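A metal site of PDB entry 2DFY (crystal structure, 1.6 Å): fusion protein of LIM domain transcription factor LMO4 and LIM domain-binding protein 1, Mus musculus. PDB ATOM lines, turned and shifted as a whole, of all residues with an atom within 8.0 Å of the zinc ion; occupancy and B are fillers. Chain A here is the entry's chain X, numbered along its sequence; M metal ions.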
ATOM      1  N   ALA A  69       5.976 -19.376  19.806  1.00  0.00           N
ATOM      2  CA  ALA A  69       7.205 -19.843  20.431  1.00  0.00           C
ATOM      3  C   ALA A  69       7.695 -21.066  19.664  1.00  0.00           C
ATOM      4  O   ALA A  69       6.876 -21.862  19.209  1.00  0.00           O
ATOM      5  CB  ALA A  69       6.932 -20.186  21.887  1.00  0.00           C
ATOM      6  N   CYS A  70       9.018 -21.188  19.518  1.00  0.00           N
ATOM      7  CA  CYS A  70       9.627 -22.273  18.729  1.00  0.00           C
ATOM      8  C   CYS A  70       9.664 -23.527  19.556  1.00  0.00           C
ATOM      9  O   CYS A  70      10.217 -23.526  20.639  1.00  0.00           O
ATOM     10  CB  CYS A  70      11.065 -21.942  18.359  1.00  0.00           C
ATOM     11  SG  CYS A  70      11.819 -23.162  17.259  1.00  0.00           S
ATOM     12  N   SER A  71       9.080 -24.600  19.031  1.00  0.00           N
ATOM     13  CA  SER A  71       9.070 -25.885  19.737  1.00  0.00           C
ATOM     14  C   SER A  71      10.475 -26.502  19.915  1.00  0.00           C
ATOM     15  O   SER A  71      10.717 -27.297  20.849  1.00  0.00           O
ATOM     16  CB  SER A  71       8.138 -26.876  19.033  1.00  0.00           C
ATOM     17  OG  SER A  71       6.783 -26.613  19.367  1.00  0.00           O
ATOM     18  N   ALA A  72      11.392 -26.148  19.015  1.00  0.00           N
ATOM     19  CA  ALA A  72      12.752 -26.656  19.059  1.00  0.00           C
ATOM     20  C   ALA A  72      13.599 -25.955  20.100  1.00  0.00           C
ATOM     21  O   ALA A  72      14.198 -26.612  20.957  1.00  0.00           O
ATOM     22  CB  ALA A  72      13.408 -26.525  17.675  1.00  0.00           C
ATOM     23  N   CYS A  73      13.666 -24.623  20.052  1.00  0.00           N
ATOM     24  CA  CYS A  73      14.565 -23.885  20.937  1.00  0.00           C
ATOM     25  C   CYS A  73      13.871 -23.184  22.113  1.00  0.00           C
ATOM     26  O   CYS A  73      14.533 -22.680  23.020  1.00  0.00           O
ATOM     27  CB  CYS A  73      15.374 -22.867  20.131  1.00  0.00           C
ATOM     28  SG  CYS A  73      14.410 -21.473  19.560  1.00  0.00           S
ATOM     29  N   GLY A  74      12.548 -23.163  22.084  1.00  0.00           N
ATOM     30  CA  GLY A  74      11.753 -22.616  23.189  1.00  0.00           C
ATOM     31  C   GLY A  74      11.566 -21.100  23.172  1.00  0.00           C
ATOM     32  O   GLY A  74      10.807 -20.579  23.987  1.00  0.00           O
ATOM     33  N   GLN A  75      12.245 -20.418  22.255  1.00  0.00           N
ATOM     34  CA  GLN A  75      12.290 -18.955  22.272  1.00  0.00           C
ATOM     35  C   GLN A  75      11.101 -18.381  21.508  1.00  0.00           C
ATOM     36  O   GLN A  75      10.646 -18.961  20.529  1.00  0.00           O
ATOM     37  CB  GLN A  75      13.588 -18.415  21.695  1.00  0.00           C
ATOM     38  CG  GLN A  75      14.877 -18.999  22.299  1.00  0.00           C
ATOM     39  CD  GLN A  75      15.021 -18.733  23.789  1.00  0.00           C
ATOM     40  OE1 GLN A  75      15.438 -17.648  24.211  1.00  0.00           O
ATOM     41  NE2 GLN A  75      14.697 -19.735  24.609  1.00  0.00           N
ATOM     42  N   SER A  76      10.608 -17.241  21.966  1.00  0.00           N
ATOM     43  CA  SER A  76       9.462 -16.584  21.340  1.00  0.00           C
ATOM     44  C   SER A  76       9.738 -16.283  19.876  1.00  0.00           C
ATOM     45  O   SER A  76      10.905 -16.083  19.485  1.00  0.00           O
ATOM     46  CB  SER A  76       9.148 -15.277  22.057  1.00  0.00           C
ATOM     47  OG  SER A  76      10.223 -14.362  21.875  1.00  0.00           O
ATOM     48  N   ILE A  77       8.675 -16.259  19.087  1.00  0.00           N
ATOM     49  CA  ILE A  77       8.732 -15.888  17.678  1.00  0.00           C
ATOM     50  C   ILE A  77       7.806 -14.685  17.474  1.00  0.00           C
ATOM     51  O   ILE A  77       6.621 -14.753  17.846  1.00  0.00           O
ATOM     52  CB  ILE A  77       8.254 -17.016  16.792  1.00  0.00           C
ATOM     53  CG1 ILE A  77       9.129 -18.270  16.978  1.00  0.00           C
ATOM     54  CG2 ILE A  77       8.243 -16.585  15.318  1.00  0.00           C
ATOM     55  CD1 ILE A  77       8.432 -19.553  16.533  1.00  0.00           C
ATOM     56  N   GLU A  81       7.482 -12.888  11.806  1.00  0.00           N
ATOM     57  CA  GLU A  81       8.497 -13.820  11.297  1.00  0.00           C
ATOM     58  C   GLU A  81       7.829 -15.002  10.603  1.00  0.00           C
ATOM     59  O   GLU A  81       6.758 -15.453  11.019  1.00  0.00           O
ATOM     60  CB  GLU A  81       9.405 -14.264  12.437  1.00  0.00           C
ATOM     61  CG  GLU A  81      10.502 -15.207  11.995  1.00  0.00           C
ATOM     62  CD  GLU A  81      11.487 -15.528  13.090  1.00  0.00           C
ATOM     63  OE1 GLU A  81      11.570 -14.795  14.102  1.00  0.00           O
ATOM     64  OE2 GLU A  81      12.199 -16.541  12.908  1.00  0.00           O
ATOM     65  N   VAL A  90       5.245 -24.823  15.876  1.00  0.00           N
ATOM     66  CA  VAL A  90       5.890 -23.876  14.994  1.00  0.00           C
ATOM     67  C   VAL A  90       7.371 -23.802  15.312  1.00  0.00           C
ATOM     68  O   VAL A  90       7.759 -23.997  16.463  1.00  0.00           O
ATOM     69  CB  VAL A  90       5.249 -22.469  15.047  1.00  0.00           C
ATOM     70  CG1 VAL A  90       3.840 -22.522  14.490  1.00  0.00           C
ATOM     71  CG2 VAL A  90       5.263 -21.900  16.433  1.00  0.00           C
ATOM     72  N   TYR A  91       8.175 -23.546  14.278  1.00  0.00           N
ATOM     73  CA  TYR A  91       9.639 -23.546  14.391  1.00  0.00           C
ATOM     74  C   TYR A  91      10.203 -22.338  13.664  1.00  0.00           C
ATOM     75  O   TYR A  91       9.638 -21.938  12.639  1.00  0.00           O
ATOM     76  CB  TYR A  91      10.215 -24.810  13.756  1.00  0.00           C
ATOM     77  CG  TYR A  91       9.683 -26.094  14.351  1.00  0.00           C
ATOM     78  CD1 TYR A  91       8.499 -26.659  13.890  1.00  0.00           C
ATOM     79  CD2 TYR A  91      10.380 -26.756  15.355  1.00  0.00           C
ATOM     80  CE1 TYR A  91       7.998 -27.849  14.432  1.00  0.00           C
ATOM     81  CE2 TYR A  91       9.883 -27.954  15.896  1.00  0.00           C
ATOM     82  CZ  TYR A  91       8.707 -28.485  15.431  1.00  0.00           C
ATOM     83  OH  TYR A  91       8.210 -29.663  15.960  1.00  0.00           O
ATOM     84  N   HIS A  92      11.295 -21.784  14.183  1.00  0.00           N
ATOM     85  CA  HIS A  92      12.177 -20.887  13.415  1.00  0.00           C
ATOM     86  C   HIS A  92      12.667 -21.641  12.210  1.00  0.00           C
ATOM     87  O   HIS A  92      12.944 -22.836  12.326  1.00  0.00           O
ATOM     88  CB  HIS A  92      13.412 -20.487  14.198  1.00  0.00           C
ATOM     89  CG  HIS A  92      13.137 -19.624  15.375  1.00  0.00           C
ATOM     90  ND1 HIS A  92      13.430 -20.010  16.672  1.00  0.00           N
ATOM     91  CD2 HIS A  92      12.634 -18.368  15.468  1.00  0.00           C
ATOM     92  CE1 HIS A  92      13.088 -19.041  17.505  1.00  0.00           C
ATOM     93  NE2 HIS A  92      12.600 -18.031  16.801  1.00  0.00           N
ATOM     94  N   LEU A  93      12.828 -20.982  11.062  1.00  0.00           N
ATOM     95  CA  LEU A  93      13.308 -21.675   9.864  1.00  0.00           C
ATOM     96  C   LEU A  93      14.606 -22.435  10.114  1.00  0.00           C
ATOM     97  O   LEU A  93      14.753 -23.603   9.711  1.00  0.00           O
ATOM     98  CB  LEU A  93      13.458 -20.713   8.661  1.00  0.00           C
ATOM     99  CG  LEU A  93      12.184 -20.531   7.855  1.00  0.00           C
ATOM    100  CD1 LEU A  93      11.115 -19.867   8.683  1.00  0.00           C
ATOM    101  CD2 LEU A  93      12.432 -19.705   6.585  1.00  0.00           C
ATOM    102  N   LYS A  94      15.534 -21.796  10.819  1.00  0.00           N
ATOM    103  CA  LYS A  94      16.833 -22.407  11.067  1.00  0.00           C
ATOM    104  C   LYS A  94      16.778 -23.443  12.187  1.00  0.00           C
ATOM    105  O   LYS A  94      17.775 -24.109  12.454  1.00  0.00           O
ATOM    106  CB  LYS A  94      17.911 -21.351  11.392  1.00  0.00           C
ATOM    107  CG  LYS A  94      18.301 -20.482  10.195  1.00  0.00           C
ATOM    108  CD  LYS A  94      19.735 -19.950  10.349  1.00  0.00           C
ATOM    109  CE  LYS A  94      20.289 -19.386   9.057  1.00  0.00           C
ATOM    110  NZ  LYS A  94      19.718 -18.057   8.748  1.00  0.00           N
ATOM    111  N   CYS A  95      15.622 -23.580  12.836  1.00  0.00           N
ATOM    112  CA  CYS A  95      15.406 -24.624  13.844  1.00  0.00           C
ATOM    113  C   CYS A  95      14.726 -25.851  13.268  1.00  0.00           C
ATOM    114  O   CYS A  95      14.664 -26.900  13.922  1.00  0.00           O
ATOM    115  CB  CYS A  95      14.602 -24.069  15.021  1.00  0.00           C
ATOM    116  SG  CYS A  95      15.582 -22.991  16.045  1.00  0.00           S
ATOM    117  N   PHE A  96      14.256 -25.750  12.038  1.00  0.00           N
ATOM    118  CA  PHE A  96      13.502 -26.812  11.441  1.00  0.00           C
ATOM    119  C   PHE A  96      14.458 -27.801  10.764  1.00  0.00           C
ATOM    120  O   PHE A  96      14.568 -27.810   9.532  1.00  0.00           O
ATOM    121  CB  PHE A  96      12.502 -26.207  10.447  1.00  0.00           C
ATOM    122  CG  PHE A  96      11.401 -27.134  10.074  1.00  0.00           C
ATOM    123  CD1 PHE A  96      10.484 -27.549  11.030  1.00  0.00           C
ATOM    124  CD2 PHE A  96      11.255 -27.588   8.773  1.00  0.00           C
ATOM    125  CE1 PHE A  96       9.454 -28.407  10.700  1.00  0.00           C
ATOM    126  CE2 PHE A  96      10.232 -28.444   8.431  1.00  0.00           C
ATOM    127  CZ  PHE A  96       9.310 -28.861   9.409  1.00  0.00           C
HETATM  128 ZN    ZN M   1      13.965 -21.949  17.367  1.00  0.00          ZN
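The zinc ion is bound by a ring nitrogen (ND1) of His 92 (2.1 Å), the side-chain sulfur of Cys 73 (2.3 Å), the side-chain sulfur of Cys 95 (2.3 Å) and the side-chain sulfur of Cys 70 (2.5 Å).
The backbone carbonyl oxygen of Cys 73 sits at hydrogen-bond distance from the side-chain amide nitrogen of Gln 75, 3.4 Å away. N of Ala 72 lies close to SG of Cys 70 (3.5 Å). N of Cys 70 is in hydrogen-bond range of O of Gln 75.
Within 4 Å of the zinc ion: Cys 70, Cys 73, His 92 and Cys 95. The nearest printed residue that does not touch the zinc ion is Ala 72 (4.6 Å).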
